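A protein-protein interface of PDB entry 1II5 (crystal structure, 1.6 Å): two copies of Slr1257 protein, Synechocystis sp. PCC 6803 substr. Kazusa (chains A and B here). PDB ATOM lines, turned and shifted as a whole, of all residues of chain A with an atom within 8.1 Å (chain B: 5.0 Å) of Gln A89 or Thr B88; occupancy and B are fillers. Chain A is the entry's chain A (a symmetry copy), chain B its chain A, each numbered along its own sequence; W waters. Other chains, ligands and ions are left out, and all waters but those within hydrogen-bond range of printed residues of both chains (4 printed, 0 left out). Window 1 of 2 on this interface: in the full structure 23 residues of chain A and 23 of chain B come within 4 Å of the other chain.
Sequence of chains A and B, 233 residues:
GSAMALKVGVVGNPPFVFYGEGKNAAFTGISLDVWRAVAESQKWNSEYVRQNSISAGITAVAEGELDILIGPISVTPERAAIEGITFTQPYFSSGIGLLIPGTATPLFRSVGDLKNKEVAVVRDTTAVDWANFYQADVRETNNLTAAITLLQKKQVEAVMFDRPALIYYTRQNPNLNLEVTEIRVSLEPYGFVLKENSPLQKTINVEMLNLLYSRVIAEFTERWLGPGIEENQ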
ATOM      1  N   VAL A  34      -3.172   2.899 -37.581  1.00  0.00           N
ATOM      2  CA  VAL A  34      -2.363   2.863 -36.359  1.00  0.00           C
ATOM      3  C   VAL A  34      -0.894   3.052 -36.719  1.00  0.00           C
ATOM      4  O   VAL A  34      -0.220   3.934 -36.179  1.00  0.00           O
ATOM      5  CB  VAL A  34      -2.538   1.536 -35.596  1.00  0.00           C
ATOM      6  CG1 VAL A  34      -1.557   1.458 -34.430  1.00  0.00           C
ATOM      7  CG2 VAL A  34      -3.961   1.414 -35.082  1.00  0.00           C
ATOM      8  N   VAL A  75      -1.497 -12.081 -30.602  1.00  0.00           N
ATOM      9  CA  VAL A  75      -0.319 -12.330 -29.770  1.00  0.00           C
ATOM     10  C   VAL A  75      -0.573 -13.664 -29.079  1.00  0.00           C
ATOM     11  O   VAL A  75      -1.412 -13.759 -28.180  1.00  0.00           O
ATOM     12  CB  VAL A  75      -0.120 -11.220 -28.692  1.00  0.00           C
ATOM     13  CG1 VAL A  75       1.183 -11.448 -27.932  1.00  0.00           C
ATOM     14  CG2 VAL A  75      -0.118  -9.839 -29.332  1.00  0.00           C
ATOM     15  N   THR A  86       9.814 -10.035 -31.269  1.00  0.00           N
ATOM     16  CA  THR A  86       9.151  -9.580 -30.061  1.00  0.00           C
ATOM     17  C   THR A  86       7.911  -8.798 -30.488  1.00  0.00           C
ATOM     18  O   THR A  86       7.939  -8.084 -31.487  1.00  0.00           O
ATOM     19  CB  THR A  86      10.068  -8.660 -29.202  1.00  0.00           C
ATOM     20  OG1 THR A  86       9.430  -8.398 -27.941  1.00  0.00           O
ATOM     21  CG2 THR A  86      10.336  -7.322 -29.908  1.00  0.00           C
ATOM     22  N   PHE A  87       6.812  -8.975 -29.761  1.00  0.00           N
ATOM     23  CA  PHE A  87       5.583  -8.245 -30.070  1.00  0.00           C
ATOM     24  C   PHE A  87       5.568  -6.883 -29.389  1.00  0.00           C
ATOM     25  O   PHE A  87       6.195  -6.695 -28.346  1.00  0.00           O
ATOM     26  CB  PHE A  87       4.362  -9.017 -29.573  1.00  0.00           C
ATOM     27  CG  PHE A  87       3.915 -10.101 -30.488  1.00  0.00           C
ATOM     28  CD1 PHE A  87       4.411 -11.392 -30.349  1.00  0.00           C
ATOM     29  CD2 PHE A  87       2.967  -9.841 -31.477  1.00  0.00           C
ATOM     30  CE1 PHE A  87       3.970 -12.410 -31.181  1.00  0.00           C
ATOM     31  CE2 PHE A  87       2.518 -10.848 -32.311  1.00  0.00           C
ATOM     32  CZ  PHE A  87       3.017 -12.139 -32.165  1.00  0.00           C
ATOM     33  N   THR A  88       4.877  -5.925 -29.996  1.00  0.00           N
ATOM     34  CA  THR A  88       4.716  -4.613 -29.384  1.00  0.00           C
ATOM     35  C   THR A  88       3.583  -4.829 -28.373  1.00  0.00           C
ATOM     36  O   THR A  88       2.997  -5.911 -28.304  1.00  0.00           O
ATOM     37  CB  THR A  88       4.163  -3.552 -30.378  1.00  0.00           C
ATOM     38  OG1 THR A  88       2.902  -4.002 -30.898  1.00  0.00           O
ATOM     39  CG2 THR A  88       5.133  -3.265 -31.509  1.00  0.00           C
ATOM     40  N   GLN A  89       3.275  -3.793 -27.601  1.00  0.00           N
ATOM     41  CA  GLN A  89       2.146  -3.845 -26.680  1.00  0.00           C
ATOM     42  C   GLN A  89       0.918  -3.987 -27.586  1.00  0.00           C
ATOM     43  O   GLN A  89       0.919  -3.484 -28.717  1.00  0.00           O
ATOM     44  CB  GLN A  89       2.041  -2.525 -25.907  1.00  0.00           C
ATOM     45  CG  GLN A  89       2.958  -2.454 -24.701  1.00  0.00           C
ATOM     46  CD  GLN A  89       2.618  -3.518 -23.686  1.00  0.00           C
ATOM     47  OE1 GLN A  89       1.453  -3.711 -23.346  1.00  0.00           O
ATOM     48  NE2 GLN A  89       3.624  -4.255 -23.238  1.00  0.00           N
ATOM     49  N   PRO A  90      -0.100  -4.750 -27.153  1.00  0.00           N
ATOM     50  CA  PRO A  90      -1.283  -4.888 -28.014  1.00  0.00           C
ATOM     51  C   PRO A  90      -2.068  -3.570 -28.160  1.00  0.00           C
ATOM     52  O   PRO A  90      -2.045  -2.720 -27.263  1.00  0.00           O
ATOM     53  CB  PRO A  90      -2.084  -6.001 -27.332  1.00  0.00           C
ATOM     54  CG  PRO A  90      -1.629  -5.947 -25.904  1.00  0.00           C
ATOM     55  CD  PRO A  90      -0.156  -5.677 -26.012  1.00  0.00           C
ATOM     56  N   TYR A  91      -2.697  -3.384 -29.322  1.00  0.00           N
ATOM     57  CA  TYR A  91      -3.457  -2.172 -29.613  1.00  0.00           C
ATOM     58  C   TYR A  91      -4.952  -2.425 -29.798  1.00  0.00           C
ATOM     59  O   TYR A  91      -5.726  -1.485 -29.990  1.00  0.00           O
ATOM     60  CB  TYR A  91      -2.897  -1.481 -30.869  1.00  0.00           C
ATOM     61  CG  TYR A  91      -3.086  -2.259 -32.157  1.00  0.00           C
ATOM     62  CD1 TYR A  91      -4.170  -1.997 -33.002  1.00  0.00           C
ATOM     63  CD2 TYR A  91      -2.203  -3.279 -32.519  1.00  0.00           C
ATOM     64  CE1 TYR A  91      -4.371  -2.734 -34.169  1.00  0.00           C
ATOM     65  CE2 TYR A  91      -2.398  -4.023 -33.684  1.00  0.00           C
ATOM     66  CZ  TYR A  91      -3.488  -3.743 -34.501  1.00  0.00           C
ATOM     67  OH  TYR A  91      -3.709  -4.486 -35.634  1.00  0.00           O
ATOM     68  N   PHE A  92      -5.356  -3.689 -29.738  1.00  0.00           N
ATOM     69  CA  PHE A  92      -6.759  -4.043 -29.920  1.00  0.00           C
ATOM     70  C   PHE A  92      -7.034  -5.389 -29.278  1.00  0.00           C
ATOM     71  O   PHE A  92      -6.190  -6.275 -29.280  1.00  0.00           O
ATOM     72  CB  PHE A  92      -7.105  -4.098 -31.422  1.00  0.00           C
ATOM     73  CG  PHE A  92      -8.585  -4.257 -31.712  1.00  0.00           C
ATOM     74  CD1 PHE A  92      -9.423  -3.144 -31.778  1.00  0.00           C
ATOM     75  CD2 PHE A  92      -9.135  -5.517 -31.932  1.00  0.00           C
ATOM     76  CE1 PHE A  92     -10.795  -3.294 -32.056  1.00  0.00           C
ATOM     77  CE2 PHE A  92     -10.498  -5.677 -32.208  1.00  0.00           C
ATOM     78  CZ  PHE A  92     -11.325  -4.565 -32.270  1.00  0.00           C
ATOM     79  N   PRO A 189      -5.446 -10.576 -28.122  1.00  0.00           N
ATOM     80  CA  PRO A 189      -4.971  -9.214 -28.352  1.00  0.00           C
ATOM     81  C   PRO A 189      -4.210  -9.157 -29.690  1.00  0.00           C
ATOM     82  O   PRO A 189      -3.629 -10.158 -30.110  1.00  0.00           O
ATOM     83  CB  PRO A 189      -4.038  -8.991 -27.164  1.00  0.00           C
ATOM     84  CG  PRO A 189      -3.437 -10.328 -26.953  1.00  0.00           C
ATOM     85  CD  PRO A 189      -4.592 -11.285 -27.151  1.00  0.00           C
ATOM     86  N   TYR A 190      -4.281  -8.020 -30.382  1.00  0.00           N
ATOM     87  CA  TYR A 190      -3.561  -7.825 -31.648  1.00  0.00           C
ATOM     88  C   TYR A 190      -2.348  -6.948 -31.369  1.00  0.00           C
ATOM     89  O   TYR A 190      -2.459  -5.952 -30.665  1.00  0.00           O
ATOM     90  CB  TYR A 190      -4.386  -7.052 -32.679  1.00  0.00           C
ATOM     91  CG  TYR A 190      -5.551  -7.764 -33.309  1.00  0.00           C
ATOM     92  CD1 TYR A 190      -6.505  -7.035 -34.009  1.00  0.00           C
ATOM     93  CD2 TYR A 190      -5.708  -9.149 -33.214  1.00  0.00           C
ATOM     94  CE1 TYR A 190      -7.584  -7.648 -34.602  1.00  0.00           C
ATOM     95  CE2 TYR A 190      -6.798  -9.786 -33.812  1.00  0.00           C
ATOM     96  CZ  TYR A 190      -7.732  -9.015 -34.504  1.00  0.00           C
ATOM     97  OH  TYR A 190      -8.838  -9.579 -35.093  1.00  0.00           O
ATOM     98  N   GLY A 191      -1.215  -7.284 -31.980  1.00  0.00           N
ATOM     99  CA  GLY A 191      -0.015  -6.486 -31.819  1.00  0.00           C
ATOM    100  C   GLY A 191       0.768  -6.485 -33.122  1.00  0.00           C
ATOM    101  O   GLY A 191       0.356  -7.106 -34.100  1.00  0.00           O
ATOM    102  N   PHE A 192       1.846  -5.713 -33.164  1.00  0.00           N
ATOM    103  CA  PHE A 192       2.716  -5.671 -34.338  1.00  0.00           C
ATOM    104  C   PHE A 192       3.957  -6.482 -33.958  1.00  0.00           C
ATOM    105  O   PHE A 192       4.202  -6.717 -32.780  1.00  0.00           O
ATOM    106  CB  PHE A 192       3.113  -4.237 -34.667  1.00  0.00           C
ATOM    107  CG  PHE A 192       1.982  -3.377 -35.176  1.00  0.00           C
ATOM    108  CD1 PHE A 192       2.120  -1.988 -35.204  1.00  0.00           C
ATOM    109  CD2 PHE A 192       0.803  -3.942 -35.659  1.00  0.00           C
ATOM    110  CE1 PHE A 192       1.114  -1.170 -35.705  1.00  0.00           C
ATOM    111  CE2 PHE A 192      -0.217  -3.127 -36.168  1.00  0.00           C
ATOM    112  CZ  PHE A 192      -0.061  -1.740 -36.191  1.00  0.00           C
ATOM    113  N   VAL A 193       4.725  -6.930 -34.942  1.00  0.00           N
ATOM    114  CA  VAL A 193       5.919  -7.724 -34.666  1.00  0.00           C
ATOM    115  C   VAL A 193       7.200  -7.004 -35.084  1.00  0.00           C
ATOM    116  O   VAL A 193       7.325  -6.514 -36.208  1.00  0.00           O
ATOM    117  CB  VAL A 193       5.860  -9.105 -35.355  1.00  0.00           C
ATOM    118  CG1 VAL A 193       7.101  -9.923 -35.022  1.00  0.00           C
ATOM    119  CG2 VAL A 193       4.607  -9.862 -34.922  1.00  0.00           C
ATOM    120  N   LEU A 194       8.140  -6.924 -34.151  1.00  0.00           N
ATOM    121  CA  LEU A 194       9.426  -6.280 -34.374  1.00  0.00           C
ATOM    122  C   LEU A 194      10.542  -7.300 -34.175  1.00  0.00           C
ATOM    123  O   LEU A 194      10.326  -8.406 -33.671  1.00  0.00           O
ATOM    124  CB  LEU A 194       9.622  -5.151 -33.361  1.00  0.00           C
ATOM    125  CG  LEU A 194       8.830  -3.851 -33.458  1.00  0.00           C
ATOM    126  CD1 LEU A 194       8.927  -3.052 -32.155  1.00  0.00           C
ATOM    127  CD2 LEU A 194       9.394  -3.051 -34.614  1.00  0.00           C
ATOM    128  N   GLN A 201      11.598  -0.378 -30.829  1.00  0.00           N
ATOM    129  CA  GLN A 201      10.632  -0.878 -29.851  1.00  0.00           C
ATOM    130  C   GLN A 201      10.023   0.119 -28.866  1.00  0.00           C
ATOM    131  O   GLN A 201       8.799   0.234 -28.783  1.00  0.00           O
ATOM    132  CB  GLN A 201      11.220  -2.072 -29.094  1.00  0.00           C
ATOM    133  CG  GLN A 201      10.267  -2.743 -28.117  1.00  0.00           C
ATOM    134  CD  GLN A 201      10.886  -3.968 -27.452  1.00  0.00           C
ATOM    135  OE1 GLN A 201      12.101  -4.162 -27.495  1.00  0.00           O
ATOM    136  NE2 GLN A 201      10.048  -4.804 -26.849  1.00  0.00           N
ATOM    137  N   ILE A 204       7.946   2.920 -30.659  1.00  0.00           N
ATOM    138  CA  ILE A 204       6.711   2.354 -31.188  1.00  0.00           C
ATOM    139  C   ILE A 204       5.707   2.067 -30.069  1.00  0.00           C
ATOM    140  O   ILE A 204       4.546   2.469 -30.167  1.00  0.00           O
ATOM    141  CB  ILE A 204       6.987   1.092 -32.041  1.00  0.00           C
ATOM    142  CG1 ILE A 204       7.726   1.503 -33.320  1.00  0.00           C
ATOM    143  CG2 ILE A 204       5.678   0.404 -32.418  1.00  0.00           C
ATOM    144  CD1 ILE A 204       8.006   0.353 -34.275  1.00  0.00           C
ATOM    145  N   ASN A 205       6.163   1.422 -28.998  1.00  0.00           N
ATOM    146  CA  ASN A 205       5.276   1.125 -27.871  1.00  0.00           C
ATOM    147  C   ASN A 205       4.693   2.400 -27.268  1.00  0.00           C
ATOM    148  O   ASN A 205       3.483   2.492 -27.045  1.00  0.00           O
ATOM    149  CB  ASN A 205       6.001   0.316 -26.795  1.00  0.00           C
ATOM    150  CG  ASN A 205       6.076  -1.153 -27.133  1.00  0.00           C
ATOM    151  OD1 ASN A 205       5.232  -1.665 -27.860  1.00  0.00           O
ATOM    152  ND2 ASN A 205       7.087  -1.842 -26.615  1.00  0.00           N
ATOM    153  N   VAL A 206       5.546   3.390 -27.025  1.00  0.00           N
ATOM    154  CA  VAL A 206       5.085   4.643 -26.448  1.00  0.00           C
ATOM    155  C   VAL A 206       4.013   5.291 -27.320  1.00  0.00           C
ATOM    156  O   VAL A 206       2.955   5.682 -26.818  1.00  0.00           O
ATOM    157  CB  VAL A 206       6.263   5.610 -26.194  1.00  0.00           C
ATOM    158  CG1 VAL A 206       5.758   6.988 -25.768  1.00  0.00           C
ATOM    159  CG2 VAL A 206       7.175   5.023 -25.122  1.00  0.00           C
ATOM    160  N   MET A 208       2.064   3.841 -29.684  1.00  0.00           N
ATOM    161  CA  MET A 208       0.863   3.023 -29.781  1.00  0.00           C
ATOM    162  C   MET A 208       0.036   3.187 -28.499  1.00  0.00           C
ATOM    163  O   MET A 208      -1.193   3.274 -28.552  1.00  0.00           O
ATOM    164  CB  MET A 208       1.235   1.557 -30.021  1.00  0.00           C
ATOM    165  CG  MET A 208       1.673   1.279 -31.459  1.00  0.00           C
ATOM    166  SD  MET A 208       2.308  -0.390 -31.707  1.00  0.00           S
ATOM    167  CE  MET A 208       0.771  -1.362 -31.638  1.00  0.00           C
ATOM    168  N   LEU A 209       0.721   3.292 -27.360  1.00  0.00           N
ATOM    169  CA  LEU A 209       0.045   3.477 -26.081  1.00  0.00           C
ATOM    170  C   LEU A 209      -0.637   4.852 -26.026  1.00  0.00           C
ATOM    171  O   LEU A 209      -1.740   4.975 -25.499  1.00  0.00           O
ATOM    172  CB  LEU A 209       1.022   3.274 -24.915  1.00  0.00           C
ATOM    173  CG  LEU A 209       1.417   1.809 -24.657  1.00  0.00           C
ATOM    174  CD1 LEU A 209       2.626   1.706 -23.739  1.00  0.00           C
ATOM    175  CD2 LEU A 209       0.235   1.049 -24.072  1.00  0.00           C
ATOM    176  N   LEU A 212      -3.704   4.658 -28.050  1.00  0.00           N
ATOM    177  CA  LEU A 212      -4.661   3.835 -27.322  1.00  0.00           C
ATOM    178  C   LEU A 212      -5.377   4.636 -26.239  1.00  0.00           C
ATOM    179  O   LEU A 212      -6.599   4.734 -26.253  1.00  0.00           O
ATOM    180  CB  LEU A 212      -3.937   2.649 -26.691  1.00  0.00           C
ATOM    181  CG  LEU A 212      -4.803   1.533 -26.126  1.00  0.00           C
ATOM    182  CD1 LEU A 212      -5.676   0.931 -27.232  1.00  0.00           C
ATOM    183  CD2 LEU A 212      -3.899   0.473 -25.502  1.00  0.00           C
ATOM    184  N   ILE A 217      -7.226   5.125 -31.391  1.00  0.00           N
ATOM    185  CA  ILE A 217      -7.402   3.807 -31.992  1.00  0.00           C
ATOM    186  C   ILE A 217      -8.894   3.457 -32.038  1.00  0.00           C
ATOM    187  O   ILE A 217      -9.375   2.876 -33.023  1.00  0.00           O
ATOM    188  CB  ILE A 217      -6.603   2.720 -31.241  1.00  0.00           C
ATOM    189  CG1 ILE A 217      -5.108   3.066 -31.271  1.00  0.00           C
ATOM    190  CG2 ILE A 217      -6.824   1.364 -31.884  1.00  0.00           C
ATOM    191  CD1 ILE A 217      -4.206   1.975 -30.761  1.00  0.00           C
ATOM    192  N   VAL B  75       0.162  -0.330 -17.653  1.00  0.00           N
ATOM    193  CA  VAL B  75       1.062  -0.057 -18.774  1.00  0.00           C
ATOM    194  C   VAL B  75       0.599   1.269 -19.366  1.00  0.00           C
ATOM    195  O   VAL B  75      -0.455   1.342 -20.002  1.00  0.00           O
ATOM    196  CB  VAL B  75       0.986  -1.166 -19.869  1.00  0.00           C
ATOM    197  CG1 VAL B  75       2.027  -0.910 -20.955  1.00  0.00           C
ATOM    198  CG2 VAL B  75       1.194  -2.544 -19.258  1.00  0.00           C
ATOM    199  N   THR B  86      11.271  -2.113 -20.097  1.00  0.00           N
ATOM    200  CA  THR B  86      10.315  -2.587 -21.081  1.00  0.00           C
ATOM    201  C   THR B  86       9.256  -3.395 -20.335  1.00  0.00           C
ATOM    202  O   THR B  86       9.572  -4.106 -19.383  1.00  0.00           O
ATOM    203  CB  THR B  86      10.984  -3.488 -22.160  1.00  0.00           C
ATOM    204  OG1 THR B  86      10.034  -3.769 -23.200  1.00  0.00           O
ATOM    205  CG2 THR B  86      11.465  -4.818 -21.558  1.00  0.00           C
ATOM    206  N   PHE B  87       7.997  -3.247 -20.734  1.00  0.00           N
ATOM    207  CA  PHE B  87       6.916  -4.003 -20.105  1.00  0.00           C
ATOM    208  C   PHE B  87       6.747  -5.368 -20.761  1.00  0.00           C
ATOM    209  O   PHE B  87       7.071  -5.545 -21.935  1.00  0.00           O
ATOM    210  CB  PHE B  87       5.588  -3.262 -20.249  1.00  0.00           C
ATOM    211  CG  PHE B  87       5.383  -2.185 -19.243  1.00  0.00           C
ATOM    212  CD1 PHE B  87       5.792  -0.884 -19.507  1.00  0.00           C
ATOM    213  CD2 PHE B  87       4.746  -2.464 -18.034  1.00  0.00           C
ATOM    214  CE1 PHE B  87       5.570   0.127 -18.584  1.00  0.00           C
ATOM    215  CE2 PHE B  87       4.518  -1.465 -17.106  1.00  0.00           C
ATOM    216  CZ  PHE B  87       4.928  -0.163 -17.378  1.00  0.00           C
ATOM    217  N   THR B  88       6.270  -6.339 -19.992  1.00  0.00           N
ATOM    218  CA  THR B  88       5.979  -7.657 -20.540  1.00  0.00           C
ATOM    219  C   THR B  88       4.608  -7.471 -21.204  1.00  0.00           C
ATOM    220  O   THR B  88       4.001  -6.402 -21.108  1.00  0.00           O
ATOM    221  CB  THR B  88       5.741  -8.727 -19.437  1.00  0.00           C
ATOM    222  OG1 THR B  88       4.660  -8.304 -18.592  1.00  0.00           O
ATOM    223  CG2 THR B  88       6.990  -8.988 -18.614  1.00  0.00           C
ATOM    224  N   GLN B  89       4.126  -8.516 -21.866  1.00  0.00           N
ATOM    225  CA  GLN B  89       2.788  -8.493 -22.445  1.00  0.00           C
ATOM    226  C   GLN B  89       1.851  -8.376 -21.239  1.00  0.00           C
ATOM    227  O   GLN B  89       2.171  -8.875 -20.153  1.00  0.00           O
ATOM    228  CB  GLN B  89       2.507  -9.817 -23.165  1.00  0.00           C
ATOM    229  CG  GLN B  89       3.062  -9.871 -24.575  1.00  0.00           C
ATOM    230  CD  GLN B  89       2.435  -8.818 -25.456  1.00  0.00           C
ATOM    231  OE1 GLN B  89       1.217  -8.653 -25.465  1.00  0.00           O
ATOM    232  NE2 GLN B  89       3.263  -8.060 -26.158  1.00  0.00           N
ATOM    233  N   PRO B  90       0.736  -7.639 -21.376  1.00  0.00           N
ATOM    234  CA  PRO B  90      -0.171  -7.525 -20.225  1.00  0.00           C
ATOM    235  C   PRO B  90      -0.856  -8.860 -19.875  1.00  0.00           C
ATOM    236  O   PRO B  90      -1.059  -9.712 -20.747  1.00  0.00           O
ATOM    237  CB  PRO B  90      -1.153  -6.433 -20.660  1.00  0.00           C
ATOM    238  CG  PRO B  90      -1.103  -6.480 -22.158  1.00  0.00           C
ATOM    239  CD  PRO B  90       0.350  -6.716 -22.456  1.00  0.00           C
ATOM    240  N   GLY B 191       0.918  -5.115 -16.419  1.00  0.00           N
ATOM    241  CA  GLY B 191       2.047  -5.886 -16.904  1.00  0.00           C
ATOM    242  C   GLY B 191       3.155  -5.864 -15.864  1.00  0.00           C
ATOM    243  O   GLY B 191       3.011  -5.250 -14.808  1.00  0.00           O
ATOM    244  N   PHE B 192       4.221  -6.612 -16.119  1.00  0.00           N
ATOM    245  CA  PHE B 192       5.379  -6.629 -15.226  1.00  0.00           C
ATOM    246  C   PHE B 192       6.450  -5.791 -15.927  1.00  0.00           C
ATOM    247  O   PHE B 192       6.360  -5.555 -17.126  1.00  0.00           O
ATOM    248  CB  PHE B 192       5.884  -8.053 -15.022  1.00  0.00           C
ATOM    249  CG  PHE B 192       4.953  -8.937 -14.227  1.00  0.00           C
ATOM    250  CD1 PHE B 192       5.126 -10.322 -14.242  1.00  0.00           C
ATOM    251  CD2 PHE B 192       3.939  -8.398 -13.440  1.00  0.00           C
ATOM    252  CE1 PHE B 192       4.313 -11.161 -13.489  1.00  0.00           C
ATOM    253  CE2 PHE B 192       3.114  -9.234 -12.675  1.00  0.00           C
ATOM    254  CZ  PHE B 192       3.303 -10.617 -12.699  1.00  0.00           C
ATOM    255  N   LEU B 194      10.517  -5.253 -16.879  1.00  0.00           N
ATOM    256  CA  LEU B 194      11.829  -5.866 -17.016  1.00  0.00           C
ATOM    257  C   LEU B 194      12.825  -4.821 -17.508  1.00  0.00           C
ATOM    258  O   LEU B 194      12.454  -3.722 -17.931  1.00  0.00           O
ATOM    259  CB  LEU B 194      11.768  -6.993 -18.048  1.00  0.00           C
ATOM    260  CG  LEU B 194      11.062  -8.311 -17.743  1.00  0.00           C
ATOM    261  CD1 LEU B 194      10.820  -9.111 -19.026  1.00  0.00           C
ATOM    262  CD2 LEU B 194      11.938  -9.094 -16.786  1.00  0.00           C
ATOM    263  N   ILE B 204       9.607 -15.109 -20.217  1.00  0.00           N
ATOM    264  CA  ILE B 204       8.549 -14.570 -19.370  1.00  0.00           C
ATOM    265  C   ILE B 204       7.273 -14.311 -20.172  1.00  0.00           C
ATOM    266  O   ILE B 204       6.192 -14.739 -19.764  1.00  0.00           O
ATOM    267  CB  ILE B 204       9.018 -13.299 -18.621  1.00  0.00           C
ATOM    268  CG1 ILE B 204      10.086 -13.689 -17.592  1.00  0.00           C
ATOM    269  CG2 ILE B 204       7.845 -12.641 -17.899  1.00  0.00           C
ATOM    270  CD1 ILE B 204      10.589 -12.530 -16.746  1.00  0.00           C
ATOM    271  N   ASN B 205       7.404 -13.658 -21.326  1.00  0.00           N
ATOM    272  CA  ASN B 205       6.238 -13.385 -22.167  1.00  0.00           C
ATOM    273  C   ASN B 205       5.542 -14.675 -22.593  1.00  0.00           C
ATOM    274  O   ASN B 205       4.320 -14.795 -22.478  1.00  0.00           O
ATOM    275  CB  ASN B 205       6.623 -12.564 -23.398  1.00  0.00           C
ATOM    276  CG  ASN B 205       6.754 -11.092 -23.088  1.00  0.00           C
ATOM    277  OD1 ASN B 205       6.128 -10.597 -22.156  1.00  0.00           O
ATOM    278  ND2 ASN B 205       7.569 -10.381 -23.860  1.00  0.00           N
ATOM    279  N   MET B 208       3.704 -16.169 -19.557  1.00  0.00           N
ATOM    280  CA  MET B 208       2.556 -15.378 -19.134  1.00  0.00           C
ATOM    281  C   MET B 208       1.416 -15.565 -20.143  1.00  0.00           C
ATOM    282  O   MET B 208       0.250 -15.680 -19.758  1.00  0.00           O
ATOM    283  CB  MET B 208       2.946 -13.904 -19.000  1.00  0.00           C
ATOM    284  CG  MET B 208       3.752 -13.611 -17.735  1.00  0.00           C
ATOM    285  SD  MET B 208       4.391 -11.927 -17.663  1.00  0.00           S
ATOM    286  CE  MET B 208       2.872 -10.991 -17.308  1.00  0.00           C
HETATM  287  O   HOH W   1       9.719 -11.271 -26.346  1.00  0.00           O
HETATM  288  O   HOH W   2       9.811  -0.895 -24.805  1.00  0.00           O
HETATM  289  O   HOH W   3       6.414  -3.866 -24.063  1.00  0.00           O
HETATM  290  O   HOH W   4       6.181  -8.381 -26.125  1.00  0.00           O
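Of the printed residues of chain B, Thr A88 touches Gln B89. Gly A191 touches none of the printed residues of chain B. Printed residues of chain B within 4 Å of Leu A209: Val B75 (3.9 Å). Thr B88 touches one residue of chain A. Of the printed residues of chain A, Pro B90 touches Gln A89 and Pro A90. Met B208 touches none of the printed residues of chain A.
NE2 of Gln A89 is in hydrogen-bond range of O of Thr B88. The backbone carbonyl oxygen (O) of Thr A88 is in hydrogen-bond range of the side-chain amide nitrogen (NE2) of Gln B89 (3.0 Å).
Among the printed residues, 11 pairs touch across the chains.
Water W4 lies within hydrogen-bond range of the backbone carbonyl oxygen of Phe A87, the side-chain amide nitrogen of Gln B89 and the side-chain amide nitrogen of Asn B205. Water W3 lies within hydrogen-bond range of the backbone carbonyl oxygen (O) of Phe B87 (2.8 Å), the side-chain amide nitrogen (NE2) of Gln A89 (2.9 Å) and the side-chain amide nitrogen (ND2) of Asn A205 (3.3 Å). Water W1 lies within hydrogen-bond range of OG1 of Thr A86 and ND2 of Asn B205. Water W2 bridges OG1 of Thr B86 and ND2 of Asn A205.
The backbone NH of Leu B194 lies within hydrogen-bond range of the backbone carbonyl oxygen of Thr B86, at 2.9 Å. The side-chain sulfur (SD) of Met B208 sits close to the side-chain hydroxyl (OG1) of Thr B88 (3.7 Å). N of Gln B89 sits at hydrogen-bond distance from OD1 of Asn B205 (2.9 Å). The side-chain hydroxyl (OG1) of Thr A88 sits close to the side-chain sulfur (SD) of Met A208 (3.7 Å). The side-chain amide oxygen (OD1) of Asn A205 sits at hydrogen-bond distance from the backbone NH (N) of Gln A89 (2.9 Å). The backbone carbonyl oxygen of Gln A201 lies close to the side-chain amide nitrogen of Asn A205, 3.5 Å away.
Val A75 touches Gln B89 (CG1 to OE1, 3.7 Å). Phe A87 touches Gln B89. CG1 of Val B75 touches OE1 of Gln A89, at 3.7 Å. Gln A89 touches Phe B87. Gln A89 touches Pro B90. OE1 of Gln B89 touches CD of Pro A90, 3.3 Å away. Pro A90 touches Pro B90. OG1 of Thr B86 touches NE2 of Gln A201, at 3.8 Å. Leu A209 touches Val B75 (CD1 to CG1, 3.9 Å).
Val A75 touches Gln B89, and with the chains exchanged Gln A89 touches Val B75. Phe A87 touches Gln B89, and with the chains exchanged Gln A89 touches Phe B87. Thr A88 touches Gln B89, and with the chains exchanged Gln A89 touches Thr B88. Gln A89 touches Pro B90, and with the chains exchanged Pro A90 touches Gln B89. Positions printed for both chains: 75, 86, 87, 88, 89, 90, 191, 192, 194, 204, 205 and 208.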
